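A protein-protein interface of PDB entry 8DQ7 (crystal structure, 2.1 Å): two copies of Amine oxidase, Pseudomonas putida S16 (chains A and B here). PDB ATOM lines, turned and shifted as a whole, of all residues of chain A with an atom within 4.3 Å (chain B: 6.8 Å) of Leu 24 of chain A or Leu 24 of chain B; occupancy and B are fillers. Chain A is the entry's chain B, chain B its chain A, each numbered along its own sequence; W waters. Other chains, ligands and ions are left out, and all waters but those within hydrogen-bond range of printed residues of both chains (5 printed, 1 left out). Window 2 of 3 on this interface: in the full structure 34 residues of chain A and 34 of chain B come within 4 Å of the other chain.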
ATOM      1  N   ARG A  20      -0.330  10.045  19.855  1.00  0.00           N
ATOM      2  CA  ARG A  20      -1.569  10.604  20.389  1.00  0.00           C
ATOM      3  C   ARG A  20      -1.904   9.982  21.754  1.00  0.00           C
ATOM      4  O   ARG A  20      -2.209  10.695  22.723  1.00  0.00           O
ATOM      5  CB  ARG A  20      -2.710  10.371  19.383  1.00  0.00           C
ATOM      6  CG  ARG A  20      -3.901  11.331  19.512  1.00  0.00           C
ATOM      7  CD  ARG A  20      -5.010  10.769  20.433  1.00  0.00           C
ATOM      8  NE  ARG A  20      -5.208   9.313  20.311  1.00  0.00           N
ATOM      9  CZ  ARG A  20      -5.990   8.738  19.403  1.00  0.00           C
ATOM     10  NH1 ARG A  20      -6.649   9.461  18.487  1.00  0.00           N
ATOM     11  NH2 ARG A  20      -6.091   7.412  19.389  1.00  0.00           N
ATOM     12  N   GLU A  21      -1.791   8.647  21.866  1.00  0.00           N
ATOM     13  CA  GLU A  21      -2.086   7.991  23.149  1.00  0.00           C
ATOM     14  C   GLU A  21      -1.141   8.474  24.238  1.00  0.00           C
ATOM     15  O   GLU A  21      -1.570   8.766  25.352  1.00  0.00           O
ATOM     16  CB  GLU A  21      -1.979   6.477  23.022  1.00  0.00           C
ATOM     17  CG  GLU A  21      -2.931   5.858  22.006  1.00  0.00           C
ATOM     18  CD  GLU A  21      -4.373   6.021  22.455  1.00  0.00           C
ATOM     19  OE1 GLU A  21      -4.781   5.306  23.386  1.00  0.00           O
ATOM     20  OE2 GLU A  21      -5.073   6.881  21.911  1.00  0.00           O
ATOM     21  N   CYS A  22       0.156   8.557  23.931  1.00  0.00           N
ATOM     22  CA  CYS A  22       1.125   8.970  24.956  1.00  0.00           C
ATOM     23  C   CYS A  22       0.961  10.439  25.330  1.00  0.00           C
ATOM     24  O   CYS A  22       1.017  10.800  26.516  1.00  0.00           O
ATOM     25  CB  CYS A  22       2.561   8.718  24.455  1.00  0.00           C
ATOM     26  SG  CYS A  22       2.911   6.933  24.218  1.00  0.00           S
ATOM     27  N   GLY A  23       0.795  11.305  24.339  1.00  0.00           N
ATOM     28  CA  GLY A  23       0.677  12.723  24.630  1.00  0.00           C
ATOM     29  C   GLY A  23      -0.545  13.032  25.473  1.00  0.00           C
ATOM     30  O   GLY A  23      -0.489  13.882  26.369  1.00  0.00           O
ATOM     31  N   LEU A  24      -1.672  12.357  25.199  1.00  0.00           N
ATOM     32  CA  LEU A  24      -2.857  12.615  26.023  1.00  0.00           C
ATOM     33  C   LEU A  24      -2.680  12.151  27.467  1.00  0.00           C
ATOM     34  O   LEU A  24      -3.435  12.596  28.343  1.00  0.00           O
ATOM     35  CB  LEU A  24      -4.094  11.939  25.422  1.00  0.00           C
ATOM     36  CG  LEU A  24      -4.579  12.606  24.116  1.00  0.00           C
ATOM     37  CD1 LEU A  24      -5.906  12.005  23.693  1.00  0.00           C
ATOM     38  CD2 LEU A  24      -4.725  14.082  24.265  1.00  0.00           C
ATOM     39  N   GLN A  25      -1.709  11.282  27.744  1.00  0.00           N
ATOM     40  CA  GLN A  25      -1.424  10.932  29.135  1.00  0.00           C
ATOM     41  C   GLN A  25      -0.525  11.939  29.802  1.00  0.00           C
ATOM     42  O   GLN A  25      -0.279  11.823  31.001  1.00  0.00           O
ATOM     43  CB  GLN A  25      -0.761   9.546  29.237  1.00  0.00           C
ATOM     44  CG  GLN A  25      -1.674   8.376  28.942  1.00  0.00           C
ATOM     45  CD  GLN A  25      -2.935   8.376  29.811  1.00  0.00           C
ATOM     46  OE1 GLN A  25      -2.850   8.471  31.032  1.00  0.00           O
ATOM     47  NE2 GLN A  25      -4.094   8.261  29.180  1.00  0.00           N
ATOM     48  N   GLY A  26      -0.036  12.942  29.067  1.00  0.00           N
ATOM     49  CA  GLY A  26       0.847  13.901  29.641  1.00  0.00           C
ATOM     50  C   GLY A  26       2.301  13.555  29.506  1.00  0.00           C
ATOM     51  O   GLY A  26       3.138  14.320  29.969  1.00  0.00           O
ATOM     52  N   ASP A 218      -3.780  16.740  18.108  1.00  0.00           N
ATOM     53  CA  ASP A 218      -4.304  16.275  19.390  1.00  0.00           C
ATOM     54  C   ASP A 218      -3.178  15.914  20.357  1.00  0.00           C
ATOM     55  O   ASP A 218      -3.256  16.223  21.553  1.00  0.00           O
ATOM     56  CB  ASP A 218      -5.195  15.048  19.136  1.00  0.00           C
ATOM     57  CG  ASP A 218      -6.325  14.922  20.125  1.00  0.00           C
ATOM     58  OD1 ASP A 218      -6.514  15.856  20.948  1.00  0.00           O
ATOM     59  OD2 ASP A 218      -7.038  13.884  20.056  1.00  0.00           O
ATOM     60  N   ALA B  19     -16.859  11.815  29.189  1.00  0.00           N
ATOM     61  CA  ALA B  19     -16.005  12.426  30.200  1.00  0.00           C
ATOM     62  C   ALA B  19     -14.545  12.092  29.959  1.00  0.00           C
ATOM     63  O   ALA B  19     -13.665  12.920  30.224  1.00  0.00           O
ATOM     64  CB  ALA B  19     -16.433  11.936  31.627  1.00  0.00           C
ATOM     65  N   ARG B  20     -14.257  10.870  29.516  1.00  0.00           N
ATOM     66  CA  ARG B  20     -12.882  10.528  29.166  1.00  0.00           C
ATOM     67  C   ARG B  20     -12.385  11.428  28.030  1.00  0.00           C
ATOM     68  O   ARG B  20     -11.311  12.043  28.128  1.00  0.00           O
ATOM     69  CB  ARG B  20     -12.815   9.050  28.777  1.00  0.00           C
ATOM     70  CG  ARG B  20     -11.422   8.402  28.892  1.00  0.00           C
ATOM     71  CD  ARG B  20     -10.630   8.455  27.596  1.00  0.00           C
ATOM     72  NE  ARG B  20     -11.450   8.268  26.374  1.00  0.00           N
ATOM     73  CZ  ARG B  20     -11.786   7.093  25.851  1.00  0.00           C
ATOM     74  NH1 ARG B  20     -11.420   5.939  26.421  1.00  0.00           N
ATOM     75  NH2 ARG B  20     -12.518   7.071  24.742  1.00  0.00           N
ATOM     76  N   GLU B  21     -13.193  11.564  26.955  1.00  0.00           N
ATOM     77  CA  GLU B  21     -12.795  12.455  25.854  1.00  0.00           C
ATOM     78  C   GLU B  21     -12.550  13.879  26.341  1.00  0.00           C
ATOM     79  O   GLU B  21     -11.568  14.505  25.957  1.00  0.00           O
ATOM     80  CB  GLU B  21     -13.851  12.463  24.757  1.00  0.00           C
ATOM     81  CG  GLU B  21     -14.125  11.076  24.163  1.00  0.00           C
ATOM     82  CD  GLU B  21     -12.908  10.583  23.401  1.00  0.00           C
ATOM     83  OE1 GLU B  21     -12.670  11.069  22.278  1.00  0.00           O
ATOM     84  OE2 GLU B  21     -12.192   9.721  23.918  1.00  0.00           O
ATOM     85  N   CYS B  22     -13.443  14.410  27.189  1.00  0.00           N
ATOM     86  CA  CYS B  22     -13.284  15.806  27.618  1.00  0.00           C
ATOM     87  C   CYS B  22     -12.101  15.974  28.571  1.00  0.00           C
ATOM     88  O   CYS B  22     -11.343  16.946  28.466  1.00  0.00           O
ATOM     89  CB  CYS B  22     -14.588  16.301  28.289  1.00  0.00           C
ATOM     90  SG  CYS B  22     -16.003  16.389  27.107  1.00  0.00           S
ATOM     91  N   GLY B  23     -11.941  15.049  29.519  1.00  0.00           N
ATOM     92  CA  GLY B  23     -10.850  15.159  30.465  1.00  0.00           C
ATOM     93  C   GLY B  23      -9.496  15.109  29.784  1.00  0.00           C
ATOM     94  O   GLY B  23      -8.590  15.863  30.146  1.00  0.00           O
ATOM     95  N   LEU B  24      -9.333  14.218  28.795  1.00  0.00           N
ATOM     96  CA  LEU B  24      -8.028  14.142  28.137  1.00  0.00           C
ATOM     97  C   LEU B  24      -7.699  15.402  27.331  1.00  0.00           C
ATOM     98  O   LEU B  24      -6.536  15.614  26.997  1.00  0.00           O
ATOM     99  CB  LEU B  24      -7.976  12.916  27.225  1.00  0.00           C
ATOM    100  CG  LEU B  24      -8.000  11.585  28.005  1.00  0.00           C
ATOM    101  CD1 LEU B  24      -7.782  10.411  27.030  1.00  0.00           C
ATOM    102  CD2 LEU B  24      -6.941  11.565  29.056  1.00  0.00           C
ATOM    103  N   GLN B  25      -8.684  16.234  27.013  1.00  0.00           N
ATOM    104  CA  GLN B  25      -8.406  17.522  26.398  1.00  0.00           C
ATOM    105  C   GLN B  25      -8.030  18.569  27.416  1.00  0.00           C
ATOM    106  O   GLN B  25      -7.665  19.674  27.023  1.00  0.00           O
ATOM    107  CB  GLN B  25      -9.602  18.039  25.592  1.00  0.00           C
ATOM    108  CG  GLN B  25      -9.940  17.245  24.346  1.00  0.00           C
ATOM    109  CD  GLN B  25      -8.773  17.173  23.360  1.00  0.00           C
ATOM    110  OE1 GLN B  25      -8.193  18.197  23.011  1.00  0.00           O
ATOM    111  NE2 GLN B  25      -8.441  15.966  22.916  1.00  0.00           N
ATOM    112  N   GLY B  26      -8.070  18.246  28.710  1.00  0.00           N
ATOM    113  CA  GLY B  26      -7.779  19.216  29.713  1.00  0.00           C
ATOM    114  C   GLY B  26      -8.976  20.015  30.188  1.00  0.00           C
ATOM    115  O   GLY B  26      -8.808  20.895  31.028  1.00  0.00           O
ATOM    116  N   TYR B  27     -10.176  19.735  29.692  1.00  0.00           N
ATOM    117  CA  TYR B  27     -11.349  20.468  30.165  1.00  0.00           C
ATOM    118  C   TYR B  27     -11.649  20.118  31.622  1.00  0.00           C
ATOM    119  O   TYR B  27     -11.574  18.948  32.025  1.00  0.00           O
ATOM    120  CB  TYR B  27     -12.570  20.148  29.317  1.00  0.00           C
ATOM    121  CG  TYR B  27     -12.393  20.430  27.849  1.00  0.00           C
ATOM    122  CD1 TYR B  27     -11.619  21.500  27.402  1.00  0.00           C
ATOM    123  CD2 TYR B  27     -13.018  19.641  26.907  1.00  0.00           C
ATOM    124  CE1 TYR B  27     -11.464  21.743  26.046  1.00  0.00           C
ATOM    125  CE2 TYR B  27     -12.860  19.882  25.559  1.00  0.00           C
ATOM    126  CZ  TYR B  27     -12.105  20.912  25.142  1.00  0.00           C
ATOM    127  OH  TYR B  27     -11.990  21.110  23.794  1.00  0.00           O
ATOM    128  N   THR B  29     -13.875  18.971  34.095  1.00  0.00           N
ATOM    129  CA  THR B  29     -15.008  18.095  33.795  1.00  0.00           C
ATOM    130  C   THR B  29     -15.626  17.530  35.059  1.00  0.00           C
ATOM    131  O   THR B  29     -14.908  17.034  35.936  1.00  0.00           O
ATOM    132  CB  THR B  29     -14.531  16.936  32.895  1.00  0.00           C
ATOM    133  OG1 THR B  29     -13.950  17.519  31.736  1.00  0.00           O
ATOM    134  CG2 THR B  29     -15.685  16.062  32.489  1.00  0.00           C
ATOM    135  N   ARG B  72      -7.487  -0.289  23.575  1.00  0.00           N
ATOM    136  CA  ARG B  72      -6.799   0.742  24.341  1.00  0.00           C
ATOM    137  C   ARG B  72      -6.490   0.282  25.775  1.00  0.00           C
ATOM    138  O   ARG B  72      -5.385   0.524  26.297  1.00  0.00           O
ATOM    139  CB  ARG B  72      -7.644   2.014  24.356  1.00  0.00           C
ATOM    140  CG  ARG B  72      -7.207   3.068  25.393  1.00  0.00           C
ATOM    141  CD  ARG B  72      -8.068   4.375  25.307  1.00  0.00           C
ATOM    142  NE  ARG B  72      -7.694   5.119  24.105  1.00  0.00           N
ATOM    143  CZ  ARG B  72      -8.463   5.234  23.017  1.00  0.00           C
ATOM    144  NH1 ARG B  72      -9.737   4.782  22.981  1.00  0.00           N
ATOM    145  NH2 ARG B  72      -7.962   5.839  21.942  1.00  0.00           N
ATOM    146  N   TYR B  73      -7.449  -0.358  26.440  1.00  0.00           N
ATOM    147  CA  TYR B  73      -7.272  -0.712  27.846  1.00  0.00           C
ATOM    148  C   TYR B  73      -6.796  -2.154  28.067  1.00  0.00           C
ATOM    149  O   TYR B  73      -6.642  -2.555  29.208  1.00  0.00           O
ATOM    150  CB  TYR B  73      -8.579  -0.443  28.606  1.00  0.00           C
ATOM    151  CG  TYR B  73      -8.866   1.043  28.627  1.00  0.00           C
ATOM    152  CD1 TYR B  73      -8.041   1.905  29.349  1.00  0.00           C
ATOM    153  CD2 TYR B  73      -9.925   1.575  27.913  1.00  0.00           C
ATOM    154  CE1 TYR B  73      -8.277   3.294  29.379  1.00  0.00           C
ATOM    155  CE2 TYR B  73     -10.192   2.963  27.929  1.00  0.00           C
ATOM    156  CZ  TYR B  73      -9.364   3.810  28.664  1.00  0.00           C
ATOM    157  OH  TYR B  73      -9.587   5.174  28.662  1.00  0.00           O
ATOM    158  N   ASP B 218      -8.982   7.225  33.750  1.00  0.00           N
ATOM    159  CA  ASP B 218      -8.290   7.917  32.671  1.00  0.00           C
ATOM    160  C   ASP B 218      -8.723   9.372  32.586  1.00  0.00           C
ATOM    161  O   ASP B 218      -7.900  10.261  32.339  1.00  0.00           O
ATOM    162  CB  ASP B 218      -8.616   7.199  31.349  1.00  0.00           C
ATOM    163  CG  ASP B 218      -7.499   7.260  30.341  1.00  0.00           C
ATOM    164  OD1 ASP B 218      -6.393   7.731  30.688  1.00  0.00           O
ATOM    165  OD2 ASP B 218      -7.752   6.808  29.199  1.00  0.00           O
ATOM    166  N   SER B 219     -10.027   9.627  32.761  1.00  0.00           N
ATOM    167  CA  SER B 219     -10.581  10.936  32.446  1.00  0.00           C
ATOM    168  C   SER B 219     -10.066  12.033  33.374  1.00  0.00           C
ATOM    169  O   SER B 219      -9.997  13.203  32.966  1.00  0.00           O
ATOM    170  CB  SER B 219     -12.095  10.896  32.535  1.00  0.00           C
ATOM    171  OG  SER B 219     -12.497  11.130  33.887  1.00  0.00           O
ATOM    172  N   GLY B 220      -9.713  11.696  34.613  1.00  0.00           N
ATOM    173  CA  GLY B 220      -9.429  12.722  35.590  1.00  0.00           C
ATOM    174  C   GLY B 220     -10.643  13.511  36.071  1.00  0.00           C
ATOM    175  O   GLY B 220     -10.484  14.384  36.933  1.00  0.00           O
HETATM  176  O   HOH W   1      -4.542  14.939  28.332  1.00  0.00           O
HETATM  177  O   HOH W   2      -5.003   9.921  32.348  1.00  0.00           O
HETATM  178  O   HOH W   3      -5.223  17.898  22.649  1.00  0.00           O
HETATM  179  O   HOH W   4      -4.599   6.416  32.913  1.00  0.00           O
HETATM  180  O   HOH W   5      -7.064   8.445  23.318  1.00  0.00           O
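NE of Arg 72 of chain B lies within salt-bridge range of OE1 of Glu 21 of chain A (3.0 Å).
The side-chain amide nitrogen (NE2) of Gln 25 of chain B lies within hydrogen-bond range of the side-chain carboxylate (OD1) of Asp 218 of chain A, 2.8 Å away.
NE2 of Gln 25 of chain A lies within hydrogen-bond range of OD1 of Asp 218 of chain B, 2.8 Å away.
OD2 of Asp 218 of chain B is in hydrogen-bond range of OH of Tyr 73 of chain B, at 2.5 Å.
NH2 of Arg 20 of chain A is in salt-bridge range of OE2 of Glu 21 of chain A (2.8 Å).
Among the printed residues, merely in contact across the chains: Arg 20 of chain A with Arg 72 of chain B (3.5 Å) and Leu 24 of chain A with Leu 24 of chain B (3.6 Å).
Of chain A, only Leu 24 (3.6 Å) comes within 4 Å of Leu 24 of chain B.
Of the printed residues of chain A, Asp 218 of chain B touches Gln 25.
Printed residues of chain A within 4 Å of Arg 72 of chain B: Arg 20 and Glu 21.
Of the 15 printed residues of chain B, 4 touch a printed residue of chain A.
Hydrophobic or aromatic side chains of chain B within 4 Å of the printed part of chain A: Leu 24.
Along chain B the printed residues that touch a printed residue of chain A span positions 24 to 218.
Of the 8 printed residues of chain A, 5 touch a printed residue of chain B.
Printed residues of chain A that touch a printed residue of chain B: Arg 20, Glu 21, Leu 24, Gln 25 and Asp 218.
Hydrophobic or aromatic side chains of chain A that line the printed part of chain B: Leu 24.
Among the printed residues, 5 pairs touch across the chains.
Among the printed residues, Asp or Glu carboxylates within 4 Å of a Lys or Arg side-chain nitrogen of the other chain: Glu 21 of chain A with Arg 72 of chain B (3.0 Å).
Leu 24 of chain A touches its own counterpart, Leu 24 of chain B.
Gln 25 of chain A touches Asp 218 of chain B, and with the chains exchanged Asp 218 of chain A touches Gln 25 of chain B.
8 positions are printed for both chains.
Water W1 lies within hydrogen-bond range of O of Leu 24 of chain B (2.5 Å) and O of Leu 24 of chain A (2.6 Å).
Water W3 bridges O of Asp 218 of chain A (2.8 Å) and OE1 of Gln 25 of chain B (3.0 Å).
Water W5 lies within hydrogen-bond range of OE2 of Glu 21 of chain A (2.9 Å) and NH2 of Arg 72 of chain B (3.1 Å).
Water W2 bridges the side-chain amide oxygen (OE1) of Gln 25 of chain A (2.9 Å) and the backbone carbonyl oxygen (O) of Asp 218 of chain B (2.9 Å).
Water W4 lies within hydrogen-bond range of OD1 of Asp 218 of chain B and OE1 of Gln 25 of chain A.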
